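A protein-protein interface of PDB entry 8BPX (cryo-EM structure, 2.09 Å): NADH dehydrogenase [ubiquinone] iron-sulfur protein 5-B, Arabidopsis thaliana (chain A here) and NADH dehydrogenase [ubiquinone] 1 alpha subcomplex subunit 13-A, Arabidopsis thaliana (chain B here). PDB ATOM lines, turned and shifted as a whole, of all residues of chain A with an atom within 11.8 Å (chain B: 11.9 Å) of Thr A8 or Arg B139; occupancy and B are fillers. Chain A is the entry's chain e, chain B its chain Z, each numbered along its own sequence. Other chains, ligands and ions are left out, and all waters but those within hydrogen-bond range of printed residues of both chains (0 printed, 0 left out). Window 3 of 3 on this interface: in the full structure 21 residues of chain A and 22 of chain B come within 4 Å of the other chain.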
ATOM      1  N   SER A   3      16.352  28.405 -36.164  1.00  0.00           N
ATOM      2  CA  SER A   3      16.910  28.757 -37.496  1.00  0.00           C
ATOM      3  C   SER A   3      17.605  27.567 -38.153  1.00  0.00           C
ATOM      4  O   SER A   3      17.660  27.550 -39.357  1.00  0.00           O
ATOM      5  CB  SER A   3      17.875  29.978 -37.388  1.00  0.00           C
ATOM      6  OG  SER A   3      19.167  29.587 -36.964  1.00  0.00           O
ATOM      7  N   GLY A   4      18.237  26.712 -37.357  1.00  0.00           N
ATOM      8  CA  GLY A   4      19.059  25.627 -37.912  1.00  0.00           C
ATOM      9  C   GLY A   4      20.536  25.912 -38.134  1.00  0.00           C
ATOM     10  O   GLY A   4      21.267  24.975 -38.318  1.00  0.00           O
ATOM     11  N   TRP A   5      20.962  27.190 -38.100  1.00  0.00           N
ATOM     12  CA  TRP A   5      22.374  27.511 -38.280  1.00  0.00           C
ATOM     13  C   TRP A   5      23.098  27.345 -36.946  1.00  0.00           C
ATOM     14  O   TRP A   5      22.848  28.098 -35.999  1.00  0.00           O
ATOM     15  CB  TRP A   5      22.541  28.930 -38.820  1.00  0.00           C
ATOM     16  CG  TRP A   5      21.807  29.227 -40.107  1.00  0.00           C
ATOM     17  CD1 TRP A   5      20.631  29.902 -40.238  1.00  0.00           C
ATOM     18  CD2 TRP A   5      22.217  28.877 -41.435  1.00  0.00           C
ATOM     19  NE1 TRP A   5      20.280  29.994 -41.560  1.00  0.00           N
ATOM     20  CE2 TRP A   5      21.236  29.373 -42.317  1.00  0.00           C
ATOM     21  CE3 TRP A   5      23.318  28.199 -41.963  1.00  0.00           C
ATOM     22  CZ2 TRP A   5      21.320  29.208 -43.697  1.00  0.00           C
ATOM     23  CZ3 TRP A   5      23.401  28.036 -43.334  1.00  0.00           C
ATOM     24  CH2 TRP A   5      22.409  28.538 -44.186  1.00  0.00           C
ATOM     25  N   GLY A   6      24.001  26.366 -36.870  1.00  0.00           N
ATOM     26  CA  GLY A   6      24.756  26.146 -35.655  1.00  0.00           C
ATOM     27  C   GLY A   6      25.965  27.059 -35.536  1.00  0.00           C
ATOM     28  O   GLY A   6      26.495  27.572 -36.518  1.00  0.00           O
ATOM     29  N   ILE A   7      26.396  27.210 -34.308  1.00  0.00           N
ATOM     30  CA  ILE A   7      27.512  28.181 -34.006  1.00  0.00           C
ATOM     31  C   ILE A   7      28.868  27.640 -34.462  1.00  0.00           C
ATOM     32  O   ILE A   7      29.753  28.424 -34.534  1.00  0.00           O
ATOM     33  CB  ILE A   7      27.447  28.649 -32.540  1.00  0.00           C
ATOM     34  CG1 ILE A   7      27.749  27.505 -31.563  1.00  0.00           C
ATOM     35  CG2 ILE A   7      26.131  29.348 -32.249  1.00  0.00           C
ATOM     36  CD1 ILE A   7      27.962  27.942 -30.144  1.00  0.00           C
ATOM     37  N   THR A   8      28.961  26.361 -34.823  1.00  0.00           N
ATOM     38  CA  THR A   8      30.198  25.775 -35.325  1.00  0.00           C
ATOM     39  C   THR A   8      30.077  25.307 -36.775  1.00  0.00           C
ATOM     40  O   THR A   8      30.934  24.561 -37.253  1.00  0.00           O
ATOM     41  CB  THR A   8      30.651  24.618 -34.431  1.00  0.00           C
ATOM     42  OG1 THR A   8      29.547  23.746 -34.169  1.00  0.00           O
ATOM     43  CG2 THR A   8      31.205  25.148 -33.110  1.00  0.00           C
ATOM     44  N   GLY A   9      29.038  25.736 -37.485  1.00  0.00           N
ATOM     45  CA  GLY A   9      28.917  25.437 -38.898  1.00  0.00           C
ATOM     46  C   GLY A   9      28.205  24.151 -39.250  1.00  0.00           C
ATOM     47  O   GLY A   9      28.345  23.679 -40.383  1.00  0.00           O
ATOM     48  N   ASN A  10      27.457  23.561 -38.322  1.00  0.00           N
ATOM     49  CA  ASN A  10      26.626  22.395 -38.595  1.00  0.00           C
ATOM     50  C   ASN A  10      25.199  22.687 -38.149  1.00  0.00           C
ATOM     51  O   ASN A  10      24.902  23.757 -37.615  1.00  0.00           O
ATOM     52  CB  ASN A  10      27.176  21.144 -37.900  1.00  0.00           C
ATOM     53  CG  ASN A  10      28.408  20.598 -38.586  1.00  0.00           C
ATOM     54  OD1 ASN A  10      28.340  20.105 -39.709  1.00  0.00           O
ATOM     55  ND2 ASN A  10      29.543  20.691 -37.915  1.00  0.00           N
ATOM     56  N   LYS A  11      24.306  21.725 -38.383  1.00  0.00           N
ATOM     57  CA  LYS A  11      22.924  21.870 -37.948  1.00  0.00           C
ATOM     58  C   LYS A  11      22.867  22.132 -36.448  1.00  0.00           C
ATOM     59  O   LYS A  11      23.582  21.504 -35.667  1.00  0.00           O
ATOM     60  CB  LYS A  11      22.115  20.615 -38.295  1.00  0.00           C
ATOM     61  CG  LYS A  11      20.711  20.598 -37.706  1.00  0.00           C
ATOM     62  CD  LYS A  11      20.104  19.196 -37.701  1.00  0.00           C
ATOM     63  CE  LYS A  11      20.016  18.623 -39.103  1.00  0.00           C
ATOM     64  NZ  LYS A  11      19.538  19.633 -40.081  1.00  0.00           N
ATOM     65  N   GLY A  12      22.090  23.142 -36.105  1.00  0.00           N
ATOM     66  CA  GLY A  12      21.870  23.472 -34.688  1.00  0.00           C
ATOM     67  C   GLY A  12      21.441  22.274 -33.838  1.00  0.00           C
ATOM     68  O   GLY A  12      20.713  21.466 -34.388  1.00  0.00           O
ATOM     69  N   ARG A  13      21.737  22.261 -32.537  1.00  0.00           N
ATOM     70  CA  ARG A  13      21.482  21.132 -31.645  1.00  0.00           C
ATOM     71  C   ARG A  13      19.998  20.787 -31.573  1.00  0.00           C
ATOM     72  O   ARG A  13      19.628  19.609 -31.576  1.00  0.00           O
ATOM     73  CB  ARG A  13      22.029  21.435 -30.247  1.00  0.00           C
ATOM     74  CG  ARG A  13      21.364  20.629 -29.131  1.00  0.00           C
ATOM     75  CD  ARG A  13      21.977  20.900 -27.764  1.00  0.00           C
ATOM     76  NE  ARG A  13      21.194  21.843 -26.976  1.00  0.00           N
ATOM     77  CZ  ARG A  13      21.580  23.083 -26.707  1.00  0.00           C
ATOM     78  NH1 ARG A  13      22.738  23.553 -27.140  1.00  0.00           N
ATOM     79  NH2 ARG A  13      20.788  23.868 -25.983  1.00  0.00           N
ATOM     80  N   CYS A  14      19.138  21.806 -31.451  1.00  0.00           N
ATOM     81  CA  CYS A  14      17.681  21.688 -31.233  1.00  0.00           C
ATOM     82  C   CYS A  14      16.807  21.850 -32.503  1.00  0.00           C
ATOM     83  O   CYS A  14      15.646  21.842 -32.375  1.00  0.00           O
ATOM     84  CB  CYS A  14      17.293  22.720 -30.186  1.00  0.00           C
ATOM     85  SG  CYS A  14      18.214  22.531 -28.645  1.00  0.00           S
ATOM     86  N   HIS A  47      17.243  22.282 -21.034  1.00  0.00           N
ATOM     87  CA  HIS A  47      17.592  21.122 -20.202  1.00  0.00           C
ATOM     88  C   HIS A  47      16.999  21.214 -18.798  1.00  0.00           C
ATOM     89  O   HIS A  47      17.615  20.769 -17.828  1.00  0.00           O
ATOM     90  CB  HIS A  47      19.109  20.928 -20.102  1.00  0.00           C
ATOM     91  CG  HIS A  47      19.834  21.075 -21.402  1.00  0.00           C
ATOM     92  ND1 HIS A  47      19.675  20.191 -22.447  1.00  0.00           N
ATOM     93  CD2 HIS A  47      20.735  21.994 -21.821  1.00  0.00           C
ATOM     94  CE1 HIS A  47      20.443  20.563 -23.455  1.00  0.00           C
ATOM     95  NE2 HIS A  47      21.095  21.654 -23.101  1.00  0.00           N
ATOM     96  N   PHE A  51      18.173  18.623 -15.709  1.00  0.00           N
ATOM     97  CA  PHE A  51      18.916  19.162 -14.578  1.00  0.00           C
ATOM     98  C   PHE A  51      18.121  19.031 -13.284  1.00  0.00           C
ATOM     99  O   PHE A  51      18.698  18.786 -12.223  1.00  0.00           O
ATOM    100  CB  PHE A  51      19.297  20.620 -14.849  1.00  0.00           C
ATOM    101  CG  PHE A  51      20.333  20.784 -15.933  1.00  0.00           C
ATOM    102  CD1 PHE A  51      21.022  19.688 -16.421  1.00  0.00           C
ATOM    103  CD2 PHE A  51      20.619  22.032 -16.459  1.00  0.00           C
ATOM    104  CE1 PHE A  51      21.968  19.828 -17.412  1.00  0.00           C
ATOM    105  CE2 PHE A  51      21.568  22.181 -17.453  1.00  0.00           C
ATOM    106  CZ  PHE A  51      22.243  21.081 -17.931  1.00  0.00           C
ATOM    107  N   TYR B  79      42.479  16.404 -44.616  1.00  0.00           N
ATOM    108  CA  TYR B  79      41.082  16.251 -44.236  1.00  0.00           C
ATOM    109  C   TYR B  79      40.587  14.856 -44.608  1.00  0.00           C
ATOM    110  O   TYR B  79      39.781  14.257 -43.886  1.00  0.00           O
ATOM    111  CB  TYR B  79      40.274  17.341 -44.934  1.00  0.00           C
ATOM    112  CG  TYR B  79      40.328  18.646 -44.180  1.00  0.00           C
ATOM    113  CD1 TYR B  79      40.355  18.677 -42.796  1.00  0.00           C
ATOM    114  CD2 TYR B  79      40.493  19.842 -44.866  1.00  0.00           C
ATOM    115  CE1 TYR B  79      40.459  19.867 -42.115  1.00  0.00           C
ATOM    116  CE2 TYR B  79      40.622  21.032 -44.195  1.00  0.00           C
ATOM    117  CZ  TYR B  79      40.595  21.042 -42.817  1.00  0.00           C
ATOM    118  OH  TYR B  79      40.706  22.233 -42.133  1.00  0.00           O
ATOM    119  N   PRO B 133      24.240  13.423 -22.590  1.00  0.00           N
ATOM    120  CA  PRO B 133      23.902  14.098 -21.331  1.00  0.00           C
ATOM    121  C   PRO B 133      24.357  15.552 -21.350  1.00  0.00           C
ATOM    122  O   PRO B 133      25.484  15.865 -21.742  1.00  0.00           O
ATOM    123  CB  PRO B 133      24.650  13.282 -20.268  1.00  0.00           C
ATOM    124  CG  PRO B 133      25.129  12.042 -20.960  1.00  0.00           C
ATOM    125  CD  PRO B 133      25.264  12.382 -22.405  1.00  0.00           C
ATOM    126  N   ALA B 134      23.462  16.440 -20.935  1.00  0.00           N
ATOM    127  CA  ALA B 134      23.791  17.854 -20.861  1.00  0.00           C
ATOM    128  C   ALA B 134      24.785  18.098 -19.731  1.00  0.00           C
ATOM    129  O   ALA B 134      24.762  17.427 -18.698  1.00  0.00           O
ATOM    130  CB  ALA B 134      22.526  18.687 -20.658  1.00  0.00           C
ATOM    131  N   THR B 135      25.667  19.075 -19.934  1.00  0.00           N
ATOM    132  CA  THR B 135      26.807  19.258 -19.049  1.00  0.00           C
ATOM    133  C   THR B 135      26.716  20.474 -18.141  1.00  0.00           C
ATOM    134  O   THR B 135      27.397  20.502 -17.113  1.00  0.00           O
ATOM    135  CB  THR B 135      28.100  19.353 -19.869  1.00  0.00           C
ATOM    136  OG1 THR B 135      28.272  20.692 -20.344  1.00  0.00           O
ATOM    137  CG2 THR B 135      28.037  18.407 -21.053  1.00  0.00           C
ATOM    138  N   GLY B 136      25.916  21.450 -18.496  1.00  0.00           N
ATOM    139  CA  GLY B 136      25.780  22.653 -17.644  1.00  0.00           C
ATOM    140  C   GLY B 136      26.971  23.599 -17.736  1.00  0.00           C
ATOM    141  O   GLY B 136      27.144  24.410 -16.846  1.00  0.00           O
ATOM    142  N   GLU B 137      27.745  23.510 -18.814  1.00  0.00           N
ATOM    143  CA  GLU B 137      28.877  24.438 -19.060  1.00  0.00           C
ATOM    144  C   GLU B 137      28.542  25.008 -20.442  1.00  0.00           C
ATOM    145  O   GLU B 137      28.174  24.244 -21.293  1.00  0.00           O
ATOM    146  CB  GLU B 137      30.257  23.786 -18.984  1.00  0.00           C
ATOM    147  CG  GLU B 137      30.683  23.393 -17.595  1.00  0.00           C
ATOM    148  CD  GLU B 137      29.984  22.138 -17.114  1.00  0.00           C
ATOM    149  OE1 GLU B 137      30.124  21.097 -17.787  1.00  0.00           O
ATOM    150  OE2 GLU B 137      29.266  22.219 -16.099  1.00  0.00           O
ATOM    151  N   LEU B 138      28.577  26.324 -20.561  1.00  0.00           N
ATOM    152  CA  LEU B 138      28.093  26.940 -21.814  1.00  0.00           C
ATOM    153  C   LEU B 138      28.936  26.516 -23.014  1.00  0.00           C
ATOM    154  O   LEU B 138      28.340  26.071 -23.979  1.00  0.00           O
ATOM    155  CB  LEU B 138      28.035  28.439 -21.591  1.00  0.00           C
ATOM    156  CG  LEU B 138      26.774  29.111 -22.115  1.00  0.00           C
ATOM    157  CD1 LEU B 138      25.529  28.408 -21.613  1.00  0.00           C
ATOM    158  CD2 LEU B 138      26.761  30.569 -21.732  1.00  0.00           C
ATOM    159  N   ARG B 139      30.251  26.657 -22.968  1.00  0.00           N
ATOM    160  CA  ARG B 139      31.131  26.384 -24.106  1.00  0.00           C
ATOM    161  C   ARG B 139      32.329  25.554 -23.659  1.00  0.00           C
ATOM    162  O   ARG B 139      33.466  26.035 -23.625  1.00  0.00           O
ATOM    163  CB  ARG B 139      31.581  27.691 -24.766  1.00  0.00           C
ATOM    164  CG  ARG B 139      32.103  27.516 -26.176  1.00  0.00           C
ATOM    165  CD  ARG B 139      31.026  27.802 -27.198  1.00  0.00           C
ATOM    166  NE  ARG B 139      31.370  27.286 -28.515  1.00  0.00           N
ATOM    167  CZ  ARG B 139      31.922  28.006 -29.482  1.00  0.00           C
ATOM    168  NH1 ARG B 139      32.220  29.284 -29.309  1.00  0.00           N
ATOM    169  NH2 ARG B 139      32.184  27.429 -30.650  1.00  0.00           N
ATOM    170  N   PRO B 140      32.107  24.281 -23.319  1.00  0.00           N
ATOM    171  CA  PRO B 140      33.230  23.451 -22.857  1.00  0.00           C
ATOM    172  C   PRO B 140      34.193  23.045 -23.961  1.00  0.00           C
ATOM    173  O   PRO B 140      35.364  22.775 -23.672  1.00  0.00           O
ATOM    174  CB  PRO B 140      32.532  22.229 -22.247  1.00  0.00           C
ATOM    175  CG  PRO B 140      31.238  22.135 -22.962  1.00  0.00           C
ATOM    176  CD  PRO B 140      30.847  23.520 -23.409  1.00  0.00           C
ATOM    177  N   ASP B 141      33.746  23.006 -25.219  1.00  0.00           N
ATOM    178  CA  ASP B 141      34.559  22.422 -26.284  1.00  0.00           C
ATOM    179  C   ASP B 141      35.728  23.302 -26.714  1.00  0.00           C
ATOM    180  O   ASP B 141      36.649  22.797 -27.362  1.00  0.00           O
ATOM    181  CB  ASP B 141      33.684  22.115 -27.499  1.00  0.00           C
ATOM    182  CG  ASP B 141      34.256  21.006 -28.361  1.00  0.00           C
ATOM    183  OD1 ASP B 141      35.077  21.306 -29.253  1.00  0.00           O
ATOM    184  OD2 ASP B 141      33.880  19.835 -28.147  1.00  0.00           O
ATOM    185  N   VAL B 142      35.726  24.597 -26.382  1.00  0.00           N
ATOM    186  CA  VAL B 142      36.784  25.487 -26.860  1.00  0.00           C
ATOM    187  C   VAL B 142      37.937  25.630 -25.875  1.00  0.00           C
ATOM    188  O   VAL B 142      38.924  26.310 -26.191  1.00  0.00           O
ATOM    189  CB  VAL B 142      36.241  26.892 -27.191  1.00  0.00           C
ATOM    190  CG1 VAL B 142      35.132  26.811 -28.230  1.00  0.00           C
ATOM    191  CG2 VAL B 142      35.763  27.589 -25.925  1.00  0.00           C
ATOM    192  N   TRP B 143      37.853  25.018 -24.701  1.00  0.00           N
ATOM    193  CA  TRP B 143      38.914  25.159 -23.708  1.00  0.00           C
ATOM    194  C   TRP B 143      39.537  23.813 -23.354  1.00  0.00           C
ATOM    195  O   TRP B 143      39.331  22.823 -24.048  1.00  0.00           O
ATOM    196  CB  TRP B 143      38.377  25.838 -22.447  1.00  0.00           C
ATOM    197  CG  TRP B 143      38.171  27.319 -22.598  1.00  0.00           C
ATOM    198  CD1 TRP B 143      36.979  27.973 -22.664  1.00  0.00           C
ATOM    199  CD2 TRP B 143      39.185  28.328 -22.697  1.00  0.00           C
ATOM    200  NE1 TRP B 143      37.182  29.322 -22.801  1.00  0.00           N
ATOM    201  CE2 TRP B 143      38.529  29.568 -22.822  1.00  0.00           C
ATOM    202  CE3 TRP B 143      40.582  28.302 -22.691  1.00  0.00           C
ATOM    203  CZ2 TRP B 143      39.221  30.771 -22.940  1.00  0.00           C
ATOM    204  CZ3 TRP B 143      41.270  29.498 -22.808  1.00  0.00           C
ATOM    205  CH2 TRP B 143      40.589  30.716 -22.934  1.00  0.00           C
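Thr A8 touches just one residue of chain B: Arg B139 (3.5 Å). Of the printed residues of chain A, Arg B139 touches Ile A7 (3.8 Å) and Thr A8 (3.5 Å). No residue of chain B comes within 4 Å of Gly A6. No residue of chain B comes within 4 Å of Asn A10. No residue of chain A comes within 4 Å of Pro B140. Of the printed residues of chain B, His A47 touches Ala B134 (3.7 Å). Of the printed residues of chain B, Phe A51 touches Ala B134 and Gly B136. Printed residues of chain A within 4 Å of Ala B134: His A47 (3.7 Å) and Phe A51 (3.5 Å). Of the printed residues of chain A, Gly B136 touches Phe A51 (3.7 Å). Ser A3 touches none of the printed residues of chain B. The nearest residue of chain A that does not touch Arg B139 is Gly A9 (7.7 Å). The nearest printed residue of chain A that does not touch Ala B134 is Arg A13 (7.2 Å).
Of the 14 printed residues of chain A, 4 touch a printed residue of chain B. Hydrophobic or aromatic side chains of chain A that line the printed part of chain B: Ile A7, His A47 and Phe A51. Of the 12 printed residues of chain B, 3 touch a printed residue of chain A. Hydrophobic or aromatic side chains of chain B within 4 Å of the printed part of chain A: Ala B134. Among the printed residues, 5 pairs touch across the chains. Among the printed residues, no Asp or Glu carboxylate lies within 4 Å of a Lys or Arg side-chain nitrogen of the other chain.
Among the printed residues, merely in contact across the chains: Phe A51 with Ala B134 (3.5 Å), Thr A8 with Arg B139 (3.5 Å), His A47 with Ala B134 (3.7 Å), Phe A51 with Gly B136 (3.7 Å) and Ile A7 with Arg B139 (3.8 Å).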
